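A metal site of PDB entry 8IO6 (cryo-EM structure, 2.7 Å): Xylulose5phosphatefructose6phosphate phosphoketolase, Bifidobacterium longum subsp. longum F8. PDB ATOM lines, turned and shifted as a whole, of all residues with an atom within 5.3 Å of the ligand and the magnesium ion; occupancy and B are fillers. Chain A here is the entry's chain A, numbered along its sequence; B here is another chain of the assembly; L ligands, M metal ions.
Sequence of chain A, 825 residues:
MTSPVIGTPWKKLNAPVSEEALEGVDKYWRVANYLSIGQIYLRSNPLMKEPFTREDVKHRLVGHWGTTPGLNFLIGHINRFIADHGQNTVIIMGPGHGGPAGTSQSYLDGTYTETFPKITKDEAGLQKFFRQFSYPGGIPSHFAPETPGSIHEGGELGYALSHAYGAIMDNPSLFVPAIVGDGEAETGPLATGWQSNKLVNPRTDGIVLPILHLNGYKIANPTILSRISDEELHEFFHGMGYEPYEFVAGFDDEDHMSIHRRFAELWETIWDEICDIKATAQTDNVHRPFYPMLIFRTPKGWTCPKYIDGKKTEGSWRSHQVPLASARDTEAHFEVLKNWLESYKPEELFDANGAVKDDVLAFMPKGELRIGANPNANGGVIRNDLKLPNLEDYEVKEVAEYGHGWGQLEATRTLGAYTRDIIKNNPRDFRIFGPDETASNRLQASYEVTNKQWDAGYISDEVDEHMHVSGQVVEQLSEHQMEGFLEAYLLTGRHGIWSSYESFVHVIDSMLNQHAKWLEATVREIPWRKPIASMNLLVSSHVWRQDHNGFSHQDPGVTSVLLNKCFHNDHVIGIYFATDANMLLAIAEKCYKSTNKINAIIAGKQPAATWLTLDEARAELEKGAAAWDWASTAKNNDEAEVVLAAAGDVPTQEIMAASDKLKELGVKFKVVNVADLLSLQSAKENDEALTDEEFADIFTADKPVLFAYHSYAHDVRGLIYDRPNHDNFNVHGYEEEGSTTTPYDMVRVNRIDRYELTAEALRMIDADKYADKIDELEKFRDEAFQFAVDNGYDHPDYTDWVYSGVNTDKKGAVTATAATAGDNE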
ATOM      1  N   GLY A  66       0.347  37.912   1.997  1.00  0.00           N
ATOM      2  CA  GLY A  66      -0.026  36.895   2.969  1.00  0.00           C
ATOM      3  C   GLY A  66       1.089  35.921   3.287  1.00  0.00           C
ATOM      4  O   GLY A  66       1.020  35.173   4.259  1.00  0.00           O
ATOM      5  N   THR A  67       2.146  35.912   2.468  1.00  0.00           N
ATOM      6  CA  THR A  67       3.276  35.043   2.731  1.00  0.00           C
ATOM      7  C   THR A  67       4.576  35.813   2.919  1.00  0.00           C
ATOM      8  O   THR A  67       5.546  35.229   3.393  1.00  0.00           O
ATOM      9  CB  THR A  67       3.444  34.038   1.585  1.00  0.00           C
ATOM     10  OG1 THR A  67       4.493  33.126   1.902  1.00  0.00           O
ATOM     11  CG2 THR A  67       3.755  34.736   0.294  1.00  0.00           C
ATOM     12  N   PRO A  95       6.037  29.243  -2.560  1.00  0.00           N
ATOM     13  CA  PRO A  95       5.069  30.305  -2.855  1.00  0.00           C
ATOM     14  C   PRO A  95       5.735  31.495  -3.529  1.00  0.00           C
ATOM     15  O   PRO A  95       6.140  32.448  -2.865  1.00  0.00           O
ATOM     16  CB  PRO A  95       4.507  30.662  -1.480  1.00  0.00           C
ATOM     17  CG  PRO A  95       4.900  29.544  -0.583  1.00  0.00           C
ATOM     18  CD  PRO A  95       6.194  29.047  -1.122  1.00  0.00           C
ATOM     19  N   HIS A  97       4.612  33.818  -5.259  1.00  0.00           N
ATOM     20  CA  HIS A  97       3.905  35.084  -5.233  1.00  0.00           C
ATOM     21  C   HIS A  97       4.398  35.978  -4.116  1.00  0.00           C
ATOM     22  O   HIS A  97       4.087  37.173  -4.088  1.00  0.00           O
ATOM     23  CB  HIS A  97       2.401  34.846  -5.099  1.00  0.00           C
ATOM     24  CG  HIS A  97       2.022  33.883  -4.023  1.00  0.00           C
ATOM     25  ND1 HIS A  97       2.037  32.520  -4.213  1.00  0.00           N
ATOM     26  CD2 HIS A  97       1.637  34.079  -2.742  1.00  0.00           C
ATOM     27  CE1 HIS A  97       1.669  31.924  -3.097  1.00  0.00           C
ATOM     28  NE2 HIS A  97       1.422  32.847  -2.191  1.00  0.00           N
ATOM     29  N   GLY A 154       7.845  29.830  -9.198  1.00  0.00           N
ATOM     30  CA  GLY A 154       6.850  29.658  -8.165  1.00  0.00           C
ATOM     31  C   GLY A 154       5.464  30.132  -8.531  1.00  0.00           C
ATOM     32  O   GLY A 154       4.570  30.059  -7.678  1.00  0.00           O
ATOM     33  N   GLY A 155       5.265  30.633  -9.741  1.00  0.00           N
ATOM     34  CA  GLY A 155       3.936  31.093 -10.119  1.00  0.00           C
ATOM     35  C   GLY A 155       2.923  29.967 -10.182  1.00  0.00           C
ATOM     36  O   GLY A 155       1.814  30.081  -9.652  1.00  0.00           O
ATOM     37  N   GLU A 156       3.301  28.873 -10.825  1.00  0.00           N
ATOM     38  CA  GLU A 156       2.433  27.714 -10.940  1.00  0.00           C
ATOM     39  C   GLU A 156       2.935  26.667  -9.948  1.00  0.00           C
ATOM     40  O   GLU A 156       4.105  26.285  -9.984  1.00  0.00           O
ATOM     41  CB  GLU A 156       2.430  27.244 -12.394  1.00  0.00           C
ATOM     42  CG  GLU A 156       1.427  26.202 -12.754  1.00  0.00           C
ATOM     43  CD  GLU A 156       1.960  24.861 -12.438  1.00  0.00           C
ATOM     44  OE1 GLU A 156       3.200  24.752 -12.490  1.00  0.00           O
ATOM     45  OE2 GLU A 156       1.193  23.929 -12.151  1.00  0.00           O
ATOM     46  N   LEU A 157       2.032  26.233  -9.065  1.00  0.00           N
ATOM     47  CA  LEU A 157       2.431  25.627  -7.796  1.00  0.00           C
ATOM     48  C   LEU A 157       2.542  24.113  -7.884  1.00  0.00           C
ATOM     49  O   LEU A 157       1.836  23.454  -8.649  1.00  0.00           O
ATOM     50  CB  LEU A 157       1.411  25.987  -6.712  1.00  0.00           C
ATOM     51  CG  LEU A 157       1.234  27.437  -6.290  1.00  0.00           C
ATOM     52  CD1 LEU A 157       0.223  27.524  -5.169  1.00  0.00           C
ATOM     53  CD2 LEU A 157       2.548  28.043  -5.860  1.00  0.00           C
ATOM     54  N   GLY A 181       4.503  26.179   0.532  1.00  0.00           N
ATOM     55  CA  GLY A 181       3.255  26.704   1.022  1.00  0.00           C
ATOM     56  C   GLY A 181       2.308  25.594   1.433  1.00  0.00           C
ATOM     57  O   GLY A 181       2.318  24.502   0.873  1.00  0.00           O
ATOM     58  N   ASP A 182       1.476  25.873   2.427  1.00  0.00           N
ATOM     59  CA  ASP A 182       0.578  24.845   2.922  1.00  0.00           C
ATOM     60  C   ASP A 182      -0.575  24.617   1.966  1.00  0.00           C
ATOM     61  O   ASP A 182      -1.119  23.507   1.897  1.00  0.00           O
ATOM     62  CB  ASP A 182       0.059  25.214   4.320  1.00  0.00           C
ATOM     63  CG  ASP A 182      -0.582  26.576   4.379  1.00  0.00           C
ATOM     64  OD1 ASP A 182      -0.460  27.356   3.420  1.00  0.00           O
ATOM     65  OD2 ASP A 182      -1.219  26.866   5.400  1.00  0.00           O
ATOM     66  N   GLY A 183      -0.977  25.649   1.228  1.00  0.00           N
ATOM     67  CA  GLY A 183      -1.934  25.444   0.158  1.00  0.00           C
ATOM     68  C   GLY A 183      -1.332  24.693  -1.016  1.00  0.00           C
ATOM     69  O   GLY A 183      -1.957  23.788  -1.568  1.00  0.00           O
ATOM     70  N   GLU A 184      -0.102  25.065  -1.394  1.00  0.00           N
ATOM     71  CA  GLU A 184       0.606  24.368  -2.448  1.00  0.00           C
ATOM     72  C   GLU A 184       0.817  22.897  -2.117  1.00  0.00           C
ATOM     73  O   GLU A 184       0.872  22.054  -3.016  1.00  0.00           O
ATOM     74  CB  GLU A 184       1.940  25.062  -2.692  1.00  0.00           C
ATOM     75  CG  GLU A 184       2.994  24.235  -3.381  1.00  0.00           C
ATOM     76  CD  GLU A 184       4.336  24.940  -3.402  1.00  0.00           C
ATOM     77  OE1 GLU A 184       4.588  25.770  -2.514  1.00  0.00           O
ATOM     78  OE2 GLU A 184       5.128  24.672  -4.327  1.00  0.00           O
ATOM     79  N   ALA A 185       0.889  22.563  -0.832  1.00  0.00           N
ATOM     80  CA  ALA A 185       1.049  21.175  -0.427  1.00  0.00           C
ATOM     81  C   ALA A 185      -0.179  20.347  -0.751  1.00  0.00           C
ATOM     82  O   ALA A 185      -0.124  19.117  -0.685  1.00  0.00           O
ATOM     83  CB  ALA A 185       1.366  21.101   1.058  1.00  0.00           C
ATOM     84  N   THR A 187      -1.561  20.468  -3.754  1.00  0.00           N
ATOM     85  CA  THR A 187      -1.462  20.139  -5.162  1.00  0.00           C
ATOM     86  C   THR A 187      -0.881  18.740  -5.342  1.00  0.00           C
ATOM     87  O   THR A 187      -0.106  18.253  -4.529  1.00  0.00           O
ATOM     88  CB  THR A 187      -0.603  21.159  -5.898  1.00  0.00           C
ATOM     89  OG1 THR A 187       0.696  21.218  -5.307  1.00  0.00           O
ATOM     90  CG2 THR A 187      -1.238  22.528  -5.836  1.00  0.00           C
ATOM     91  N   HIS A 213       5.597  26.044   5.078  1.00  0.00           N
ATOM     92  CA  HIS A 213       5.191  27.386   5.503  1.00  0.00           C
ATOM     93  C   HIS A 213       3.690  27.361   5.743  1.00  0.00           C
ATOM     94  O   HIS A 213       2.881  27.797   4.931  1.00  0.00           O
ATOM     95  CB  HIS A 213       5.606  28.404   4.450  1.00  0.00           C
ATOM     96  CG  HIS A 213       5.117  29.787   4.719  1.00  0.00           C
ATOM     97  ND1 HIS A 213       5.386  30.466   5.883  1.00  0.00           N
ATOM     98  CD2 HIS A 213       4.443  30.655   3.924  1.00  0.00           C
ATOM     99  CE1 HIS A 213       4.851  31.674   5.830  1.00  0.00           C
ATOM    100  NE2 HIS A 213       4.282  31.807   4.645  1.00  0.00           N
ATOM    101  N   ASN A 215       0.891  28.686   7.146  1.00  0.00           N
ATOM    102  CA  ASN A 215       0.197  29.843   7.683  1.00  0.00           C
ATOM    103  C   ASN A 215      -1.322  29.676   7.692  1.00  0.00           C
ATOM    104  O   ASN A 215      -2.026  30.616   8.062  1.00  0.00           O
ATOM    105  CB  ASN A 215       0.592  31.118   6.936  1.00  0.00           C
ATOM    106  CG  ASN A 215       0.433  31.022   5.439  1.00  0.00           C
ATOM    107  OD1 ASN A 215      -0.270  30.165   4.928  1.00  0.00           O
ATOM    108  ND2 ASN A 215       1.076  31.917   4.730  1.00  0.00           N
ATOM    109  N   GLY A 216      -1.824  28.513   7.320  1.00  0.00           N
ATOM    110  CA  GLY A 216      -3.206  28.158   7.540  1.00  0.00           C
ATOM    111  C   GLY A 216      -4.181  28.404   6.423  1.00  0.00           C
ATOM    112  O   GLY A 216      -5.266  27.832   6.416  1.00  0.00           O
ATOM    113  N   TYR A 217      -3.821  29.259   5.469  1.00  0.00           N
ATOM    114  CA  TYR A 217      -4.767  29.731   4.482  1.00  0.00           C
ATOM    115  C   TYR A 217      -4.179  29.735   3.075  1.00  0.00           C
ATOM    116  O   TYR A 217      -2.992  29.978   2.867  1.00  0.00           O
ATOM    117  CB  TYR A 217      -5.270  31.127   4.833  1.00  0.00           C
ATOM    118  CG  TYR A 217      -5.845  31.183   6.215  1.00  0.00           C
ATOM    119  CD1 TYR A 217      -7.140  30.780   6.468  1.00  0.00           C
ATOM    120  CD2 TYR A 217      -5.077  31.611   7.282  1.00  0.00           C
ATOM    121  CE1 TYR A 217      -7.653  30.809   7.728  1.00  0.00           C
ATOM    122  CE2 TYR A 217      -5.585  31.638   8.533  1.00  0.00           C
ATOM    123  CZ  TYR A 217      -6.860  31.239   8.762  1.00  0.00           C
ATOM    124  OH  TYR A 217      -7.359  31.278  10.039  1.00  0.00           O
ATOM    125  N   LYS A 218      -5.062  29.427   2.132  1.00  0.00           N
ATOM    126  CA  LYS A 218      -4.921  29.649   0.706  1.00  0.00           C
ATOM    127  C   LYS A 218      -5.499  31.019   0.360  1.00  0.00           C
ATOM    128  O   LYS A 218      -5.591  31.884   1.234  1.00  0.00           O
ATOM    129  CB  LYS A 218      -5.640  28.555  -0.077  1.00  0.00           C
ATOM    130  CG  LYS A 218      -5.210  27.173   0.304  1.00  0.00           C
ATOM    131  CD  LYS A 218      -5.790  26.143  -0.631  1.00  0.00           C
ATOM    132  CE  LYS A 218      -7.269  25.918  -0.428  1.00  0.00           C
ATOM    133  NZ  LYS A 218      -7.547  25.136   0.791  1.00  0.00           N
ATOM    134  N   ILE A 219      -5.839  31.255  -0.898  1.00  0.00           N
ATOM    135  CA  ILE A 219      -6.712  32.356  -1.274  1.00  0.00           C
ATOM    136  C   ILE A 219      -8.102  32.009  -0.770  1.00  0.00           C
ATOM    137  O   ILE A 219      -8.712  31.046  -1.247  1.00  0.00           O
ATOM    138  CB  ILE A 219      -6.752  32.576  -2.801  1.00  0.00           C
ATOM    139  CG1 ILE A 219      -5.361  32.797  -3.366  1.00  0.00           C
ATOM    140  CG2 ILE A 219      -7.615  33.773  -3.129  1.00  0.00           C
ATOM    141  CD1 ILE A 219      -5.342  32.772  -4.867  1.00  0.00           C
ATOM    142  N   THR A 223      -6.276  25.698   4.583  1.00  0.00           N
ATOM    143  CA  THR A 223      -5.572  24.547   4.040  1.00  0.00           C
ATOM    144  C   THR A 223      -5.878  23.302   4.854  1.00  0.00           C
ATOM    145  O   THR A 223      -6.101  23.368   6.062  1.00  0.00           O
ATOM    146  CB  THR A 223      -4.073  24.811   4.015  1.00  0.00           C
ATOM    147  OG1 THR A 223      -3.572  24.868   5.351  1.00  0.00           O
ATOM    148  CG2 THR A 223      -3.798  26.117   3.347  1.00  0.00           C
ATOM    149  N   LYS A 300      -0.872  34.256   8.762  1.00  0.00           N
ATOM    150  CA  LYS A 300      -0.766  34.839   7.432  1.00  0.00           C
ATOM    151  C   LYS A 300      -0.769  36.354   7.500  1.00  0.00           C
ATOM    152  O   LYS A 300      -1.629  36.956   8.137  1.00  0.00           O
ATOM    153  CB  LYS A 300      -1.920  34.328   6.578  1.00  0.00           C
ATOM    154  CG  LYS A 300      -1.843  34.710   5.125  1.00  0.00           C
ATOM    155  CD  LYS A 300      -2.562  33.701   4.260  1.00  0.00           C
ATOM    156  CE  LYS A 300      -2.308  33.974   2.807  1.00  0.00           C
ATOM    157  NZ  LYS A 300      -2.643  32.805   1.974  1.00  0.00           N
ATOM    158  N   HIS A 320      -4.166  37.830   1.914  1.00  0.00           N
ATOM    159  CA  HIS A 320      -3.429  37.140   0.851  1.00  0.00           C
ATOM    160  C   HIS A 320      -2.807  38.123  -0.126  1.00  0.00           C
ATOM    161  O   HIS A 320      -1.578  38.256  -0.189  1.00  0.00           O
ATOM    162  CB  HIS A 320      -4.354  36.178   0.117  1.00  0.00           C
ATOM    163  CG  HIS A 320      -3.710  35.495  -1.045  1.00  0.00           C
ATOM    164  ND1 HIS A 320      -2.777  34.485  -0.893  1.00  0.00           N
ATOM    165  CD2 HIS A 320      -3.849  35.674  -2.378  1.00  0.00           C
ATOM    166  CE1 HIS A 320      -2.384  34.077  -2.077  1.00  0.00           C
ATOM    167  NE2 HIS A 320      -3.000  34.781  -2.998  1.00  0.00           N
ATOM    168  N   PRO B 435     -10.549  25.000  -7.834  1.00  0.00           N
ATOM    169  CA  PRO B 435      -9.244  24.880  -7.165  1.00  0.00           C
ATOM    170  C   PRO B 435      -8.856  26.144  -6.410  1.00  0.00           C
ATOM    171  O   PRO B 435      -7.913  26.855  -6.759  1.00  0.00           O
ATOM    172  CB  PRO B 435      -8.305  24.594  -8.341  1.00  0.00           C
ATOM    173  CG  PRO B 435      -8.960  25.224  -9.503  1.00  0.00           C
ATOM    174  CD  PRO B 435     -10.422  25.051  -9.298  1.00  0.00           C
ATOM    175  N   ASP B 436      -9.608  26.418  -5.336  1.00  0.00           N
ATOM    176  CA  ASP B 436      -9.396  27.563  -4.451  1.00  0.00           C
ATOM    177  C   ASP B 436      -9.752  28.884  -5.105  1.00  0.00           C
ATOM    178  O   ASP B 436      -9.321  29.952  -4.652  1.00  0.00           O
ATOM    179  CB  ASP B 436      -7.958  27.572  -3.925  1.00  0.00           C
ATOM    180  CG  ASP B 436      -7.731  28.588  -2.839  1.00  0.00           C
ATOM    181  OD1 ASP B 436      -8.450  28.516  -1.817  1.00  0.00           O
ATOM    182  OD2 ASP B 436      -6.843  29.455  -2.989  1.00  0.00           O
ATOM    183  N   GLU B 437     -10.576  28.868  -6.154  1.00  0.00           N
ATOM    184  CA  GLU B 437     -10.738  30.031  -7.009  1.00  0.00           C
ATOM    185  C   GLU B 437     -12.200  30.387  -7.295  1.00  0.00           C
ATOM    186  O   GLU B 437     -12.456  31.186  -8.202  1.00  0.00           O
ATOM    187  CB  GLU B 437      -9.984  29.779  -8.317  1.00  0.00           C
ATOM    188  CG  GLU B 437      -8.476  29.728  -8.101  1.00  0.00           C
ATOM    189  CD  GLU B 437      -7.709  29.451  -9.352  1.00  0.00           C
ATOM    190  OE1 GLU B 437      -8.359  29.169 -10.388  1.00  0.00           O
ATOM    191  OE2 GLU B 437      -6.474  29.515  -9.319  1.00  0.00           O
ATOM    192  N   LEU B 477      -7.127  23.031  -3.358  1.00  0.00           N
ATOM    193  CA  LEU B 477      -6.111  23.574  -4.253  1.00  0.00           C
ATOM    194  C   LEU B 477      -5.425  22.442  -5.007  1.00  0.00           C
ATOM    195  O   LEU B 477      -4.296  22.049  -4.740  1.00  0.00           O
ATOM    196  CB  LEU B 477      -5.110  24.417  -3.481  1.00  0.00           C
ATOM    197  CG  LEU B 477      -4.007  25.083  -4.312  1.00  0.00           C
ATOM    198  CD1 LEU B 477      -4.590  25.671  -5.566  1.00  0.00           C
ATOM    199  CD2 LEU B 477      -3.335  26.139  -3.492  1.00  0.00           C
ATOM    200  N   GLU B 479      -6.151  21.047  -9.217  1.00  0.00           N
ATOM    201  CA  GLU B 479      -7.011  20.927 -10.397  1.00  0.00           C
ATOM    202  C   GLU B 479      -7.327  19.473 -10.700  1.00  0.00           C
ATOM    203  O   GLU B 479      -8.424  19.167 -11.184  1.00  0.00           O
ATOM    204  CB  GLU B 479      -6.382  21.593 -11.609  1.00  0.00           C
ATOM    205  CG  GLU B 479      -6.013  23.081 -11.444  1.00  0.00           C
ATOM    206  CD  GLU B 479      -4.849  23.338 -10.486  1.00  0.00           C
ATOM    207  OE1 GLU B 479      -3.760  22.757 -10.698  1.00  0.00           O
ATOM    208  OE2 GLU B 479      -5.030  24.122  -9.533  1.00  0.00           O
ATOM    209  N   TYR B 501      -8.686  29.337 -13.306  1.00  0.00           N
ATOM    210  CA  TYR B 501      -7.810  30.223 -14.068  1.00  0.00           C
ATOM    211  C   TYR B 501      -7.490  29.591 -15.408  1.00  0.00           C
ATOM    212  O   TYR B 501      -7.392  28.365 -15.527  1.00  0.00           O
ATOM    213  CB  TYR B 501      -6.511  30.456 -13.309  1.00  0.00           C
ATOM    214  CG  TYR B 501      -6.558  31.499 -12.218  1.00  0.00           C
ATOM    215  CD1 TYR B 501      -7.753  31.834 -11.598  1.00  0.00           C
ATOM    216  CD2 TYR B 501      -5.406  32.109 -11.774  1.00  0.00           C
ATOM    217  CE1 TYR B 501      -7.797  32.769 -10.592  1.00  0.00           C
ATOM    218  CE2 TYR B 501      -5.437  33.045 -10.761  1.00  0.00           C
ATOM    219  CZ  TYR B 501      -6.636  33.367 -10.176  1.00  0.00           C
ATOM    220  OH  TYR B 501      -6.668  34.293  -9.174  1.00  0.00           O
ATOM    221  N   PHE B 504      -3.959  27.578 -15.747  1.00  0.00           N
ATOM    222  CA  PHE B 504      -3.771  26.327 -15.025  1.00  0.00           C
ATOM    223  C   PHE B 504      -4.676  25.207 -15.515  1.00  0.00           C
ATOM    224  O   PHE B 504      -4.562  24.086 -15.016  1.00  0.00           O
ATOM    225  CB  PHE B 504      -3.968  26.553 -13.528  1.00  0.00           C
ATOM    226  CG  PHE B 504      -3.089  27.626 -12.976  1.00  0.00           C
ATOM    227  CD1 PHE B 504      -1.757  27.677 -13.315  1.00  0.00           C
ATOM    228  CD2 PHE B 504      -3.596  28.604 -12.156  1.00  0.00           C
ATOM    229  CE1 PHE B 504      -0.938  28.661 -12.841  1.00  0.00           C
ATOM    230  CE2 PHE B 504      -2.771  29.596 -11.679  1.00  0.00           C
ATOM    231  CZ  PHE B 504      -1.451  29.617 -12.019  1.00  0.00           C
ATOM    232  N   VAL B 507      -2.964  22.066 -16.449  1.00  0.00           N
ATOM    233  CA  VAL B 507      -2.665  21.042 -15.446  1.00  0.00           C
ATOM    234  C   VAL B 507      -3.490  19.787 -15.707  1.00  0.00           C
ATOM    235  O   VAL B 507      -3.045  18.676 -15.419  1.00  0.00           O
ATOM    236  CB  VAL B 507      -2.907  21.610 -14.041  1.00  0.00           C
ATOM    237  CG1 VAL B 507      -2.887  20.519 -12.999  1.00  0.00           C
ATOM    238  CG2 VAL B 507      -1.869  22.661 -13.720  1.00  0.00           C
ATOM    239  N   HIS B 553       1.100  33.475 -15.016  1.00  0.00           N
ATOM    240  CA  HIS B 553      -0.307  33.109 -15.016  1.00  0.00           C
ATOM    241  C   HIS B 553      -0.993  33.370 -16.344  1.00  0.00           C
ATOM    242  O   HIS B 553      -2.231  33.426 -16.387  1.00  0.00           O
ATOM    243  CB  HIS B 553      -1.040  33.849 -13.913  1.00  0.00           C
ATOM    244  CG  HIS B 553      -0.723  33.354 -12.534  1.00  0.00           C
ATOM    245  ND1 HIS B 553       0.541  33.416 -11.998  1.00  0.00           N
ATOM    246  CD2 HIS B 553      -1.507  32.799 -11.588  1.00  0.00           C
ATOM    247  CE1 HIS B 553       0.526  32.909 -10.780  1.00  0.00           C
ATOM    248  NE2 HIS B 553      -0.710  32.519 -10.506  1.00  0.00           N
HETATM  249  N1  LIG L   1      -3.361  26.568  -9.013  1.00  0.00           N
HETATM  250  C1  LIG L   1      -2.056  26.383  -9.260  1.00  0.00           C
HETATM  251  C2  LIG L   1      -1.631  25.014  -9.682  1.00  0.00           C
HETATM  252  N2  LIG L   1      -1.096  27.302  -9.136  1.00  0.00           N
HETATM  253  C3  LIG L   1      -1.466  28.537  -8.753  1.00  0.00           C
HETATM  254  N3  LIG L   1      -0.490  29.447  -8.642  1.00  0.00           N
HETATM  255  C4  LIG L   1      -2.821  28.841  -8.473  1.00  0.00           C
HETATM  256  C5  LIG L   1      -3.701  27.804  -8.626  1.00  0.00           C
HETATM  257  C6  LIG L   1      -3.279  30.205  -8.034  1.00  0.00           C
HETATM  258  N4  LIG L   1      -2.659  30.655  -6.775  1.00  0.00           N
HETATM  259  C7  LIG L   1      -1.675  31.530  -6.700  1.00  0.00           C
HETATM  260  S1  LIG L   1      -1.197  31.815  -5.135  1.00  0.00           S
HETATM  261  C8  LIG L   1      -2.372  30.710  -4.529  1.00  0.00           C
HETATM  262  C9  LIG L   1      -3.061  30.167  -5.533  1.00  0.00           C
HETATM  263  C10 LIG L   1      -4.173  29.175  -5.430  1.00  0.00           C
HETATM  264  C11 LIG L   1      -2.507  30.445  -3.057  1.00  0.00           C
HETATM  265  C12 LIG L   1      -1.181  30.191  -2.378  1.00  0.00           C
HETATM  266  O1  LIG L   1      -1.353  29.095  -1.443  1.00  0.00           O
HETATM  267  P1  LIG L   1      -0.308  28.734  -0.338  1.00  0.00           P
HETATM  268  O2  LIG L   1       0.693  27.772  -0.849  1.00  0.00           O
HETATM  269  O3  LIG L   1      -1.023  28.362   0.930  1.00  0.00           O
HETATM  270  O4  LIG L   1       0.339  30.103  -0.090  1.00  0.00           O
HETATM  271  P2  LIG L   1       0.431  31.195   1.048  1.00  0.00           P
HETATM  272  O5  LIG L   1       1.895  31.331   1.313  1.00  0.00           O
HETATM  273  O6  LIG L   1      -0.363  30.776   2.233  1.00  0.00           O
HETATM  274  O7  LIG L   1      -0.058  32.449   0.400  1.00  0.00           O
HETATM  275 MG    MG M   1      -0.911  29.293   3.286  1.00  0.00          MG
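A nitrogen (N2) of the ligand is in hydrogen-bond range of the backbone NH of Leu 157, 3.3 Å away. A ring nitrogen (NE2) of His 97 lies within hydrogen-bond range of an oxygen (O7) of the ligand (3.0 Å). N3 of the ligand sits at hydrogen-bond distance from O of Gly 155, at 2.6 Å. OG1 of Thr 67 sits close to O5 of the ligand, 3.2 Å away. The backbone NH of Glu 184 sits at hydrogen-bond distance from an oxygen (O2) of the ligand (2.9 Å). The backbone NH of Gly 183 sits at hydrogen-bond distance from an oxygen (O2) of the ligand (3.4 Å). O7 of the ligand lies within salt-bridge range of NZ of Lys 300.
The backbone carbonyl oxygen (O) of Glu 184 lies within hydrogen-bond range of the side-chain hydroxyl (OG1) of Thr 187. The backbone carbonyl oxygen (O) of Leu 477 of chain B sits close to the backbone NH (N) of Thr 187 (3.3 Å). OE1 of Glu 184 lies within hydrogen-bond range of N of Gly 181, at 3.1 Å. The side-chain amino group of Lys 300 lies within hydrogen-bond range of the backbone carbonyl oxygen of Lys 218. The side-chain amide nitrogen of Asn 215 is in hydrogen-bond range of a ring nitrogen (NE2) of His 213, at 3.2 Å. N of Ile 219 is in hydrogen-bond range of OD2 of Asp 436 of chain B. N of Asp 182 is in hydrogen-bond range of O of His 213 (3.5 Å). The side-chain amide nitrogen of Asn 215 is in hydrogen-bond range of the backbone carbonyl oxygen of Gly 66 (3.3 Å).
OE2 of Glu 479 of chain B sits close to N1 of the ligand, at 3.0 Å. Merely in contact with the ligand: Pro 95 (3.9 Å), Glu 156 (3.9 Å), Gly 181 (3.3 Å), His 213 (3.7 Å), Ile 219 (3.5 Å), His 320 (3.6 Å), Asp 436 of chain B (3.6 Å), Glu 437 of chain B (3.3 Å), Leu 477 of chain B (3.5 Å), Phe 504 of chain B (3.3 Å) and His 553 of chain B (3.6 Å). Hydrophobic or aromatic side chains within 4 Å of the ligand: Pro 95, His 97, Leu 157, His 213, Ile 219, His 320, Leu 477 of chain B and Phe 504 of chain B. 22 residues have an atom within 4 Å of the ligand: Thr 67, Pro 95, His 97, Gly 155, Glu 156, Leu 157, Gly 181, Asp 182, Gly 183, Glu 184, His 213, Asn 215, Tyr 217, Ile 219, Lys 300, His 320, Asp 436 of chain B, Glu 437 of chain B, Leu 477 of chain B, Glu 479 of chain B, Phe 504 of chain B and His 553 of chain B. The nearest printed residue that does not touch the ligand is Lys 218 (4.1 Å).
The nearest printed residue that does not touch the magnesium ion is Lys 300 (4.1 Å).
The magnesium ion is bound by O6 of the ligand (1.9 Å), OD1 of Asn 215 (2.0 Å), OD1 of Asp 182 (2.0 Å), O of Tyr 217 (2.2 Å) and O3 of the ligand (2.5 Å).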
